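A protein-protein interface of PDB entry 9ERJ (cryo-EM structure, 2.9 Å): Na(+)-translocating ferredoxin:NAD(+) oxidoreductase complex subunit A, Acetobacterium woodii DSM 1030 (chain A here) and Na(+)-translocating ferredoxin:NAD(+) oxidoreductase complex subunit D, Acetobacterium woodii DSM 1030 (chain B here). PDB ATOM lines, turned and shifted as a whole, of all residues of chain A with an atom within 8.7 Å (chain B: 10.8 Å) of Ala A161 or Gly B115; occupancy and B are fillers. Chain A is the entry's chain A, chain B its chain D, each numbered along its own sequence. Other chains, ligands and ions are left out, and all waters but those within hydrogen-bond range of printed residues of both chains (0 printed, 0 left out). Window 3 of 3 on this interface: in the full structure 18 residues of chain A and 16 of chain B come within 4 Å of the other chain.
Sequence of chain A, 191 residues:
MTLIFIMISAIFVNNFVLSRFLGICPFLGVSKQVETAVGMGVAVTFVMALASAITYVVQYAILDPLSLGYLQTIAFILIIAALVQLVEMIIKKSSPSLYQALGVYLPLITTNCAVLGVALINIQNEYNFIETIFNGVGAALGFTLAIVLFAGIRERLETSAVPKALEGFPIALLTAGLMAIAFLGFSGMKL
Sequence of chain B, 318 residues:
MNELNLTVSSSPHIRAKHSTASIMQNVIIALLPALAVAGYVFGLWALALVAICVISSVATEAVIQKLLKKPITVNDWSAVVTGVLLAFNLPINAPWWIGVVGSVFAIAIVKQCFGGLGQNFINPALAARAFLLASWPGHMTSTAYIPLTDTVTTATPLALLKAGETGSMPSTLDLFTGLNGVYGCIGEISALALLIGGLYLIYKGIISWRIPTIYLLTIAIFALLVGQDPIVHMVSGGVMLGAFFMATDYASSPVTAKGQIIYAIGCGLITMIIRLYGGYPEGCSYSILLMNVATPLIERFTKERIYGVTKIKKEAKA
The backbone carbonyl oxygen (O) of Ala B108 lies within hydrogen-bond range of the side-chain sulfur (SG) of Cys B113 (3.4 Å).
NH2 of Arg A156 touches O of Gly B118 (3.7 Å). Phe B121 touches Arg A156. CD2 of Leu A157 touches CD2 of Phe B114 (3.7 Å). Ala A161 touches Phe B114. Ala A161 touches Gly B115 (O to CA, 3.3 Å). O of Cys B113 touches CD1 of Leu A166 (3.4 Å). O of Cys B113 touches CD1 of Ile A171 (3.7 Å).
Printed residues of chain B within 4 Å of Leu A157: Phe B114 (3.7 Å). Ala A161 touches two residues of chain B. Lys A164 touches none of the printed residues of chain B. Pro B71 touches none of the printed residues of chain A. Of the printed residues of chain A, Cys B113 touches Leu A166 (3.4 Å) and Ile A171 (3.7 Å). Printed residues of chain A within 4 Å of Phe B114: Leu A157 and Ala A161. Gly B115 touches one residue of chain A. No residue of chain A comes within 4 Å of Gly B116. Of the printed residues of chain A, Ala B251 touches Arg A156 (3.0 Å). The nearest residue of chain B that does not touch Ala A161 is Gln B119 (4.3 Å).
NH1 of Arg A156 is in hydrogen-bond range of O of Asn B120, 3.3 Å away. NH1 of Arg A156 sits at hydrogen-bond distance from O of Ala B251 (3.0 Å). The side-chain hydroxyl (OG) of Ser A160 lies within hydrogen-bond range of the backbone carbonyl oxygen (O) of Gln B119 (3.1 Å).
Printed residues of chain B that touch a printed residue of chain A: Cys B113, Phe B114, Gly B115, Gly B118, Gln B119, Asn B120, Phe B121 and Ala B251. Hydrophobic or aromatic side chains of chain B that line the printed part of chain A: Phe B114 and Phe B121. Of the 13 printed residues of chain A, 6 touch a printed residue of chain B. Printed residues of chain A that touch a printed residue of chain B: Arg A156, Leu A157, Ser A160, Ala A161, Leu A166 and Ile A171. Hydrophobic or aromatic side chains of chain A that line the printed part of chain B: Leu A157, Leu A166 and Ile A171.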
ATOM      1  N   ARG A 156      24.881   5.626   8.831  1.00  0.00           N
ATOM      2  CA  ARG A 156      25.799   4.540   8.500  1.00  0.00           C
ATOM      3  C   ARG A 156      25.105   3.191   8.609  1.00  0.00           C
ATOM      4  O   ARG A 156      25.390   2.273   7.832  1.00  0.00           O
ATOM      5  CB  ARG A 156      27.033   4.591   9.405  1.00  0.00           C
ATOM      6  CG  ARG A 156      28.252   3.864   8.840  1.00  0.00           C
ATOM      7  CD  ARG A 156      28.325   2.429   9.345  1.00  0.00           C
ATOM      8  NE  ARG A 156      29.211   1.589   8.550  1.00  0.00           N
ATOM      9  CZ  ARG A 156      30.428   1.215   8.923  1.00  0.00           C
ATOM     10  NH1 ARG A 156      30.953   1.617  10.067  1.00  0.00           N
ATOM     11  NH2 ARG A 156      31.131   0.415   8.130  1.00  0.00           N
ATOM     12  N   LEU A 157      24.187   3.049   9.569  1.00  0.00           N
ATOM     13  CA  LEU A 157      23.389   1.829   9.625  1.00  0.00           C
ATOM     14  C   LEU A 157      22.449   1.692   8.434  1.00  0.00           C
ATOM     15  O   LEU A 157      22.209   0.568   7.980  1.00  0.00           O
ATOM     16  CB  LEU A 157      22.586   1.769  10.926  1.00  0.00           C
ATOM     17  CG  LEU A 157      23.367   1.465  12.202  1.00  0.00           C
ATOM     18  CD1 LEU A 157      22.421   0.993  13.292  1.00  0.00           C
ATOM     19  CD2 LEU A 157      24.446   0.425  11.941  1.00  0.00           C
ATOM     20  N   GLU A 158      21.904   2.799   7.924  1.00  0.00           N
ATOM     21  CA  GLU A 158      21.039   2.718   6.749  1.00  0.00           C
ATOM     22  C   GLU A 158      21.840   2.319   5.515  1.00  0.00           C
ATOM     23  O   GLU A 158      21.291   1.764   4.557  1.00  0.00           O
ATOM     24  CB  GLU A 158      20.306   4.045   6.522  1.00  0.00           C
ATOM     25  CG  GLU A 158      20.861   4.915   5.401  1.00  0.00           C
ATOM     26  CD  GLU A 158      20.094   6.209   5.230  1.00  0.00           C
ATOM     27  OE1 GLU A 158      19.009   6.343   5.831  1.00  0.00           O
ATOM     28  OE2 GLU A 158      20.578   7.092   4.492  1.00  0.00           O
ATOM     29  N   THR A 159      23.143   2.601   5.517  1.00  0.00           N
ATOM     30  CA  THR A 159      24.019   2.057   4.480  1.00  0.00           C
ATOM     31  C   THR A 159      24.152   0.535   4.559  1.00  0.00           C
ATOM     32  O   THR A 159      24.128  -0.129   3.516  1.00  0.00           O
ATOM     33  CB  THR A 159      25.403   2.724   4.564  1.00  0.00           C
ATOM     34  OG1 THR A 159      25.367   3.989   3.892  1.00  0.00           O
ATOM     35  CG2 THR A 159      26.488   1.864   3.929  1.00  0.00           C
ATOM     36  N   SER A 160      24.240  -0.033   5.765  1.00  0.00           N
ATOM     37  CA  SER A 160      24.420  -1.470   5.956  1.00  0.00           C
ATOM     38  C   SER A 160      23.139  -2.247   5.677  1.00  0.00           C
ATOM     39  O   SER A 160      22.144  -1.673   5.223  1.00  0.00           O
ATOM     40  CB  SER A 160      24.902  -1.759   7.378  1.00  0.00           C
ATOM     41  OG  SER A 160      26.209  -1.256   7.588  1.00  0.00           O
ATOM     42  N   ALA A 161      23.146  -3.556   5.954  1.00  0.00           N
ATOM     43  CA  ALA A 161      22.039  -4.444   5.602  1.00  0.00           C
ATOM     44  C   ALA A 161      21.610  -5.264   6.825  1.00  0.00           C
ATOM     45  O   ALA A 161      22.074  -6.386   7.030  1.00  0.00           O
ATOM     46  CB  ALA A 161      22.426  -5.354   4.436  1.00  0.00           C
ATOM     47  N   VAL A 162      20.709  -4.703   7.630  1.00  0.00           N
ATOM     48  CA  VAL A 162      20.062  -5.521   8.664  1.00  0.00           C
ATOM     49  C   VAL A 162      19.143  -6.524   7.980  1.00  0.00           C
ATOM     50  O   VAL A 162      18.552  -6.196   6.930  1.00  0.00           O
ATOM     51  CB  VAL A 162      19.293  -4.636   9.660  1.00  0.00           C
ATOM     52  CG1 VAL A 162      20.261  -3.765  10.435  1.00  0.00           C
ATOM     53  CG2 VAL A 162      18.274  -3.767   8.943  1.00  0.00           C
ATOM     54  N   PRO A 163      19.013  -7.774   8.483  1.00  0.00           N
ATOM     55  CA  PRO A 163      18.515  -8.855   7.615  1.00  0.00           C
ATOM     56  C   PRO A 163      17.099  -8.686   7.076  1.00  0.00           C
ATOM     57  O   PRO A 163      16.940  -8.380   5.889  1.00  0.00           O
ATOM     58  CB  PRO A 163      18.596 -10.088   8.527  1.00  0.00           C
ATOM     59  CG  PRO A 163      19.591  -9.734   9.577  1.00  0.00           C
ATOM     60  CD  PRO A 163      19.425  -8.271   9.807  1.00  0.00           C
ATOM     61  N   LYS A 164      16.069  -8.869   7.904  1.00  0.00           N
ATOM     62  CA  LYS A 164      14.730  -8.424   7.532  1.00  0.00           C
ATOM     63  C   LYS A 164      13.889  -8.067   8.751  1.00  0.00           C
ATOM     64  O   LYS A 164      12.894  -7.344   8.641  1.00  0.00           O
ATOM     65  CB  LYS A 164      14.025  -9.495   6.696  1.00  0.00           C
ATOM     66  CG  LYS A 164      12.819  -8.981   5.924  1.00  0.00           C
ATOM     67  CD  LYS A 164      13.247  -8.209   4.687  1.00  0.00           C
ATOM     68  CE  LYS A 164      12.045  -7.759   3.876  1.00  0.00           C
ATOM     69  NZ  LYS A 164      10.882  -7.432   4.747  1.00  0.00           N
ATOM     70  N   ALA A 165      14.289  -8.564   9.921  1.00  0.00           N
ATOM     71  CA  ALA A 165      13.393  -8.614  11.068  1.00  0.00           C
ATOM     72  C   ALA A 165      13.762  -7.644  12.176  1.00  0.00           C
ATOM     73  O   ALA A 165      12.894  -7.297  12.984  1.00  0.00           O
ATOM     74  CB  ALA A 165      13.346 -10.033  11.647  1.00  0.00           C
ATOM     75  N   LEU A 166      15.015  -7.199  12.238  1.00  0.00           N
ATOM     76  CA  LEU A 166      15.388  -6.215  13.251  1.00  0.00           C
ATOM     77  C   LEU A 166      14.915  -4.829  12.823  1.00  0.00           C
ATOM     78  O   LEU A 166      14.008  -4.258  13.435  1.00  0.00           O
ATOM     79  CB  LEU A 166      16.901  -6.256  13.483  1.00  0.00           C
ATOM     80  CG  LEU A 166      17.439  -7.632  13.892  1.00  0.00           C
ATOM     81  CD1 LEU A 166      18.923  -7.571  14.185  1.00  0.00           C
ATOM     82  CD2 LEU A 166      16.686  -8.178  15.093  1.00  0.00           C
ATOM     83  N   GLU A 167      15.472  -4.317  11.724  1.00  0.00           N
ATOM     84  CA  GLU A 167      15.065  -3.062  11.067  1.00  0.00           C
ATOM     85  C   GLU A 167      15.013  -1.935  12.100  1.00  0.00           C
ATOM     86  O   GLU A 167      16.036  -1.660  12.742  1.00  0.00           O
ATOM     87  CB  GLU A 167      13.775  -3.313  10.300  1.00  0.00           C
ATOM     88  CG  GLU A 167      13.935  -4.261   9.115  1.00  0.00           C
ATOM     89  CD  GLU A 167      14.408  -3.574   7.842  1.00  0.00           C
ATOM     90  OE1 GLU A 167      15.061  -2.513   7.928  1.00  0.00           O
ATOM     91  OE2 GLU A 167      14.128  -4.102   6.747  1.00  0.00           O
ATOM     92  N   ILE A 171      17.307  -2.688  16.152  1.00  0.00           N
ATOM     93  CA  ILE A 171      18.683  -2.282  15.883  1.00  0.00           C
ATOM     94  C   ILE A 171      18.997  -0.968  16.592  1.00  0.00           C
ATOM     95  O   ILE A 171      20.138  -0.743  17.014  1.00  0.00           O
ATOM     96  CB  ILE A 171      18.958  -2.222  14.365  1.00  0.00           C
ATOM     97  CG1 ILE A 171      20.351  -2.773  14.064  1.00  0.00           C
ATOM     98  CG2 ILE A 171      18.886  -0.805  13.824  1.00  0.00           C
ATOM     99  CD1 ILE A 171      20.518  -4.230  14.409  1.00  0.00           C
ATOM    100  N   GLU B  61      29.921 -18.824  13.615  1.00  0.00           N
ATOM    101  CA  GLU B  61      29.616 -18.216  12.328  1.00  0.00           C
ATOM    102  C   GLU B  61      28.941 -19.224  11.419  1.00  0.00           C
ATOM    103  O   GLU B  61      27.853 -18.957  10.887  1.00  0.00           O
ATOM    104  CB  GLU B  61      30.893 -17.670  11.690  1.00  0.00           C
ATOM    105  CG  GLU B  61      30.695 -17.068  10.313  1.00  0.00           C
ATOM    106  CD  GLU B  61      31.639 -15.913  10.048  1.00  0.00           C
ATOM    107  OE1 GLU B  61      32.861 -16.089  10.231  1.00  0.00           O
ATOM    108  OE2 GLU B  61      31.161 -14.827   9.660  1.00  0.00           O
ATOM    109  N   ILE B  64      25.250 -19.862  12.232  1.00  0.00           N
ATOM    110  CA  ILE B  64      24.361 -18.782  11.831  1.00  0.00           C
ATOM    111  C   ILE B  64      24.194 -18.784  10.322  1.00  0.00           C
ATOM    112  O   ILE B  64      23.074 -18.678   9.805  1.00  0.00           O
ATOM    113  CB  ILE B  64      24.884 -17.433  12.355  1.00  0.00           C
ATOM    114  CG1 ILE B  64      24.828 -17.408  13.884  1.00  0.00           C
ATOM    115  CG2 ILE B  64      24.069 -16.287  11.780  1.00  0.00           C
ATOM    116  CD1 ILE B  64      25.195 -16.077  14.492  1.00  0.00           C
ATOM    117  N   GLN B  65      25.291 -19.010   9.593  1.00  0.00           N
ATOM    118  CA  GLN B  65      25.211 -18.961   8.140  1.00  0.00           C
ATOM    119  C   GLN B  65      24.479 -20.178   7.593  1.00  0.00           C
ATOM    120  O   GLN B  65      24.125 -20.216   6.411  1.00  0.00           O
ATOM    121  CB  GLN B  65      26.611 -18.836   7.543  1.00  0.00           C
ATOM    122  CG  GLN B  65      26.954 -17.415   7.129  1.00  0.00           C
ATOM    123  CD  GLN B  65      28.438 -17.199   6.941  1.00  0.00           C
ATOM    124  OE1 GLN B  65      29.237 -18.122   7.087  1.00  0.00           O
ATOM    125  NE2 GLN B  65      28.819 -15.969   6.620  1.00  0.00           N
ATOM    126  N   LEU B  68      20.286 -18.997   8.401  1.00  0.00           N
ATOM    127  CA  LEU B  68      19.698 -17.880   7.675  1.00  0.00           C
ATOM    128  C   LEU B  68      19.662 -18.108   6.168  1.00  0.00           C
ATOM    129  O   LEU B  68      19.271 -17.199   5.428  1.00  0.00           O
ATOM    130  CB  LEU B  68      20.459 -16.591   7.988  1.00  0.00           C
ATOM    131  CG  LEU B  68      19.783 -15.613   8.950  1.00  0.00           C
ATOM    132  CD1 LEU B  68      19.630 -16.233  10.327  1.00  0.00           C
ATOM    133  CD2 LEU B  68      20.566 -14.316   9.031  1.00  0.00           C
ATOM    134  N   LYS B  69      20.059 -19.297   5.706  1.00  0.00           N
ATOM    135  CA  LYS B  69      20.105 -19.655   4.284  1.00  0.00           C
ATOM    136  C   LYS B  69      20.994 -18.687   3.499  1.00  0.00           C
ATOM    137  O   LYS B  69      20.554 -17.987   2.586  1.00  0.00           O
ATOM    138  CB  LYS B  69      18.696 -19.732   3.685  1.00  0.00           C
ATOM    139  CG  LYS B  69      17.706 -20.512   4.532  1.00  0.00           C
ATOM    140  CD  LYS B  69      16.292 -20.386   3.992  1.00  0.00           C
ATOM    141  CE  LYS B  69      15.340 -21.325   4.715  1.00  0.00           C
ATOM    142  NZ  LYS B  69      15.955 -21.928   5.930  1.00  0.00           N
ATOM    143  N   LYS B  70      22.264 -18.666   3.875  1.00  0.00           N
ATOM    144  CA  LYS B  70      23.287 -17.828   3.273  1.00  0.00           C
ATOM    145  C   LYS B  70      24.485 -18.688   2.911  1.00  0.00           C
ATOM    146  O   LYS B  70      24.687 -19.760   3.493  1.00  0.00           O
ATOM    147  CB  LYS B  70      23.721 -16.709   4.232  1.00  0.00           C
ATOM    148  CG  LYS B  70      22.744 -15.556   4.337  1.00  0.00           C
ATOM    149  CD  LYS B  70      23.278 -14.474   5.257  1.00  0.00           C
ATOM    150  CE  LYS B  70      22.292 -13.328   5.386  1.00  0.00           C
ATOM    151  NZ  LYS B  70      22.816 -12.234   6.248  1.00  0.00           N
ATOM    152  N   PRO B  71      25.285 -18.265   1.930  1.00  0.00           N
ATOM    153  CA  PRO B  71      26.535 -18.980   1.647  1.00  0.00           C
ATOM    154  C   PRO B  71      27.471 -18.949   2.847  1.00  0.00           C
ATOM    155  O   PRO B  71      27.579 -17.941   3.547  1.00  0.00           O
ATOM    156  CB  PRO B  71      27.121 -18.213   0.456  1.00  0.00           C
ATOM    157  CG  PRO B  71      25.949 -17.556  -0.184  1.00  0.00           C
ATOM    158  CD  PRO B  71      25.014 -17.213   0.935  1.00  0.00           C
ATOM    159  N   THR B  73      30.653 -18.417   3.997  1.00  0.00           N
ATOM    160  CA  THR B  73      31.924 -17.785   3.641  1.00  0.00           C
ATOM    161  C   THR B  73      32.861 -17.755   4.847  1.00  0.00           C
ATOM    162  O   THR B  73      33.301 -16.703   5.306  1.00  0.00           O
ATOM    163  CB  THR B  73      31.682 -16.382   3.096  1.00  0.00           C
ATOM    164  OG1 THR B  73      30.974 -15.605   4.069  1.00  0.00           O
ATOM    165  CG2 THR B  73      30.865 -16.442   1.815  1.00  0.00           C
ATOM    166  N   ASP B  76      37.302 -16.910   4.496  1.00  0.00           N
ATOM    167  CA  ASP B  76      37.952 -15.613   4.376  1.00  0.00           C
ATOM    168  C   ASP B  76      38.815 -15.273   5.584  1.00  0.00           C
ATOM    169  O   ASP B  76      39.384 -14.180   5.631  1.00  0.00           O
ATOM    170  CB  ASP B  76      36.912 -14.510   4.146  1.00  0.00           C
ATOM    171  CG  ASP B  76      35.791 -14.537   5.164  1.00  0.00           C
ATOM    172  OD1 ASP B  76      35.797 -15.420   6.044  1.00  0.00           O
ATOM    173  OD2 ASP B  76      34.898 -13.669   5.083  1.00  0.00           O
ATOM    174  N   ALA B 106      30.975 -11.966  20.763  1.00  0.00           N
ATOM    175  CA  ALA B 106      31.638 -11.163  19.740  1.00  0.00           C
ATOM    176  C   ALA B 106      31.110 -11.478  18.346  1.00  0.00           C
ATOM    177  O   ALA B 106      30.951 -10.571  17.522  1.00  0.00           O
ATOM    178  CB  ALA B 106      33.149 -11.381  19.799  1.00  0.00           C
ATOM    179  N   ILE B 107      30.836 -12.747  18.058  1.00  0.00           N
ATOM    180  CA  ILE B 107      30.425 -13.134  16.710  1.00  0.00           C
ATOM    181  C   ILE B 107      28.923 -12.974  16.512  1.00  0.00           C
ATOM    182  O   ILE B 107      28.479 -12.393  15.519  1.00  0.00           O
ATOM    183  CB  ILE B 107      30.881 -14.578  16.413  1.00  0.00           C
ATOM    184  CG1 ILE B 107      32.408 -14.655  16.364  1.00  0.00           C
ATOM    185  CG2 ILE B 107      30.282 -15.069  15.106  1.00  0.00           C
ATOM    186  CD1 ILE B 107      33.015 -14.007  15.142  1.00  0.00           C
ATOM    187  N   ALA B 108      28.113 -13.481  17.445  1.00  0.00           N
ATOM    188  CA  ALA B 108      26.672 -13.548  17.217  1.00  0.00           C
ATOM    189  C   ALA B 108      26.017 -12.174  17.302  1.00  0.00           C
ATOM    190  O   ALA B 108      25.189 -11.820  16.455  1.00  0.00           O
ATOM    191  CB  ALA B 108      26.031 -14.510  18.217  1.00  0.00           C
ATOM    192  N   ILE B 109      26.370 -11.385  18.311  1.00  0.00           N
ATOM    193  CA  ILE B 109      25.637 -10.154  18.602  1.00  0.00           C
ATOM    194  C   ILE B 109      26.238  -8.955  17.882  1.00  0.00           C
ATOM    195  O   ILE B 109      25.532  -8.218  17.188  1.00  0.00           O
ATOM    196  CB  ILE B 109      25.578  -9.925  20.128  1.00  0.00           C
ATOM    197  CG1 ILE B 109      24.572 -10.879  20.768  1.00  0.00           C
ATOM    198  CG2 ILE B 109      25.206  -8.485  20.446  1.00  0.00           C
ATOM    199  CD1 ILE B 109      24.464 -10.738  22.265  1.00  0.00           C
ATOM    200  N   VAL B 110      27.543  -8.728  18.038  1.00  0.00           N
ATOM    201  CA  VAL B 110      28.158  -7.525  17.483  1.00  0.00           C
ATOM    202  C   VAL B 110      28.224  -7.598  15.962  1.00  0.00           C
ATOM    203  O   VAL B 110      27.890  -6.631  15.266  1.00  0.00           O
ATOM    204  CB  VAL B 110      29.549  -7.307  18.105  1.00  0.00           C
ATOM    205  CG1 VAL B 110      30.333  -6.284  17.313  1.00  0.00           C
ATOM    206  CG2 VAL B 110      29.418  -6.868  19.552  1.00  0.00           C
ATOM    207  N   LYS B 111      28.632  -8.743  15.418  1.00  0.00           N
ATOM    208  CA  LYS B 111      28.949  -8.843  13.996  1.00  0.00           C
ATOM    209  C   LYS B 111      27.748  -9.260  13.151  1.00  0.00           C
ATOM    210  O   LYS B 111      27.357  -8.546  12.223  1.00  0.00           O
ATOM    211  CB  LYS B 111      30.110  -9.824  13.798  1.00  0.00           C
ATOM    212  CG  LYS B 111      30.662  -9.863  12.387  1.00  0.00           C
ATOM    213  CD  LYS B 111      31.779 -10.883  12.272  1.00  0.00           C
ATOM    214  CE  LYS B 111      32.259 -11.021  10.841  1.00  0.00           C
ATOM    215  NZ  LYS B 111      33.284 -12.086  10.705  1.00  0.00           N
ATOM    216  N   GLN B 112      27.153 -10.415  13.458  1.00  0.00           N
ATOM    217  CA  GLN B 112      26.158 -11.011  12.574  1.00  0.00           C
ATOM    218  C   GLN B 112      24.770 -10.400  12.708  1.00  0.00           C
ATOM    219  O   GLN B 112      23.921 -10.654  11.847  1.00  0.00           O
ATOM    220  CB  GLN B 112      26.072 -12.518  12.819  1.00  0.00           C
ATOM    221  CG  GLN B 112      27.346 -13.272  12.480  1.00  0.00           C
ATOM    222  CD  GLN B 112      27.493 -13.525  10.996  1.00  0.00           C
ATOM    223  OE1 GLN B 112      26.505 -13.610  10.268  1.00  0.00           O
ATOM    224  NE2 GLN B 112      28.731 -13.645  10.536  1.00  0.00           N
ATOM    225  N   CYS B 113      24.505  -9.613  13.751  1.00  0.00           N
ATOM    226  CA  CYS B 113      23.206  -8.963  13.868  1.00  0.00           C
ATOM    227  C   CYS B 113      23.106  -7.699  13.028  1.00  0.00           C
ATOM    228  O   CYS B 113      21.994  -7.207  12.805  1.00  0.00           O
ATOM    229  CB  CYS B 113      22.904  -8.629  15.331  1.00  0.00           C
ATOM    230  SG  CYS B 113      22.284 -10.016  16.306  1.00  0.00           S
ATOM    231  N   PHE B 114      24.232  -7.163  12.562  1.00  0.00           N
ATOM    232  CA  PHE B 114      24.249  -5.960  11.744  1.00  0.00           C
ATOM    233  C   PHE B 114      24.413  -6.251  10.260  1.00  0.00           C
ATOM    234  O   PHE B 114      24.469  -5.312   9.463  1.00  0.00           O
ATOM    235  CB  PHE B 114      25.364  -5.020  12.211  1.00  0.00           C
ATOM    236  CG  PHE B 114      25.045  -4.284  13.481  1.00  0.00           C
ATOM    237  CD1 PHE B 114      25.198  -4.899  14.711  1.00  0.00           C
ATOM    238  CD2 PHE B 114      24.592  -2.977  13.444  1.00  0.00           C
ATOM    239  CE1 PHE B 114      24.903  -4.225  15.880  1.00  0.00           C
ATOM    240  CE2 PHE B 114      24.297  -2.300  14.609  1.00  0.00           C
ATOM    241  CZ  PHE B 114      24.453  -2.925  15.828  1.00  0.00           C
ATOM    242  N   GLY B 115      24.495  -7.521   9.870  1.00  0.00           N
ATOM    243  CA  GLY B 115      24.613  -7.870   8.469  1.00  0.00           C
ATOM    244  C   GLY B 115      25.730  -8.842   8.149  1.00  0.00           C
ATOM    245  O   GLY B 115      25.575  -9.703   7.279  1.00  0.00           O
ATOM    246  N   GLY B 116      26.863  -8.719   8.837  1.00  0.00           N
ATOM    247  CA  GLY B 116      27.984  -9.602   8.586  1.00  0.00           C
ATOM    248  C   GLY B 116      29.324  -8.900   8.548  1.00  0.00           C
ATOM    249  O   GLY B 116      29.577  -7.988   9.340  1.00  0.00           O
ATOM    250  N   LEU B 117      30.191  -9.318   7.628  1.00  0.00           N
ATOM    251  CA  LEU B 117      31.537  -8.765   7.548  1.00  0.00           C
ATOM    252  C   LEU B 117      31.510  -7.342   7.003  1.00  0.00           C
ATOM    253  O   LEU B 117      30.912  -7.077   5.956  1.00  0.00           O
ATOM    254  CB  LEU B 117      32.414  -9.649   6.663  1.00  0.00           C
ATOM    255  CG  LEU B 117      33.814  -9.135   6.324  1.00  0.00           C
ATOM    256  CD1 LEU B 117      34.696  -9.101   7.559  1.00  0.00           C
ATOM    257  CD2 LEU B 117      34.445  -9.987   5.240  1.00  0.00           C
ATOM    258  N   GLY B 118      32.165  -6.429   7.715  1.00  0.00           N
ATOM    259  CA  GLY B 118      32.296  -5.061   7.258  1.00  0.00           C
ATOM    260  C   GLY B 118      31.065  -4.200   7.410  1.00  0.00           C
ATOM    261  O   GLY B 118      31.045  -3.082   6.888  1.00  0.00           O
ATOM    262  N   GLN B 119      30.037  -4.677   8.112  1.00  0.00           N
ATOM    263  CA  GLN B 119      28.779  -3.949   8.230  1.00  0.00           C
ATOM    264  C   GLN B 119      28.465  -3.522   9.658  1.00  0.00           C
ATOM    265  O   GLN B 119      27.363  -3.027   9.914  1.00  0.00           O
ATOM    266  CB  GLN B 119      27.631  -4.786   7.664  1.00  0.00           C
ATOM    267  CG  GLN B 119      27.320  -4.458   6.218  1.00  0.00           C
ATOM    268  CD  GLN B 119      27.195  -5.686   5.352  1.00  0.00           C
ATOM    269  OE1 GLN B 119      26.835  -6.759   5.828  1.00  0.00           O
ATOM    270  NE2 GLN B 119      27.503  -5.537   4.072  1.00  0.00           N
ATOM    271  N   ASN B 120      29.393  -3.697  10.590  1.00  0.00           N
ATOM    272  CA  ASN B 120      29.242  -3.190  11.944  1.00  0.00           C
ATOM    273  C   ASN B 120      29.973  -1.859  12.090  1.00  0.00           C
ATOM    274  O   ASN B 120      30.789  -1.472  11.252  1.00  0.00           O
ATOM    275  CB  ASN B 120      29.761  -4.207  12.964  1.00  0.00           C
ATOM    276  CG  ASN B 120      31.127  -4.748  12.604  1.00  0.00           C
ATOM    277  OD1 ASN B 120      31.636  -4.505  11.513  1.00  0.00           O
ATOM    278  ND2 ASN B 120      31.734  -5.480  13.527  1.00  0.00           N
ATOM    279  N   PHE B 121      29.666  -1.152  13.176  1.00  0.00           N
ATOM    280  CA  PHE B 121      30.276   0.140  13.457  1.00  0.00           C
ATOM    281  C   PHE B 121      31.166   0.127  14.691  1.00  0.00           C
ATOM    282  O   PHE B 121      31.723   1.171  15.044  1.00  0.00           O
ATOM    283  CB  PHE B 121      29.190   1.217  13.606  1.00  0.00           C
ATOM    284  CG  PHE B 121      28.416   1.135  14.896  1.00  0.00           C
ATOM    285  CD1 PHE B 121      27.387   0.220  15.045  1.00  0.00           C
ATOM    286  CD2 PHE B 121      28.705   1.985  15.953  1.00  0.00           C
ATOM    287  CE1 PHE B 121      26.673   0.144  16.224  1.00  0.00           C
ATOM    288  CE2 PHE B 121      27.995   1.911  17.135  1.00  0.00           C
ATOM    289  CZ  PHE B 121      26.978   0.990  17.270  1.00  0.00           C
ATOM    290  N   ALA B 251      36.481  -1.635   9.419  1.00  0.00           N
ATOM    291  CA  ALA B 251      35.072  -1.264   9.452  1.00  0.00           C
ATOM    292  C   ALA B 251      34.742  -0.223  10.514  1.00  0.00           C
ATOM    293  O   ALA B 251      33.575   0.164  10.629  1.00  0.00           O
ATOM    294  CB  ALA B 251      34.209  -2.508   9.675  1.00  0.00           C
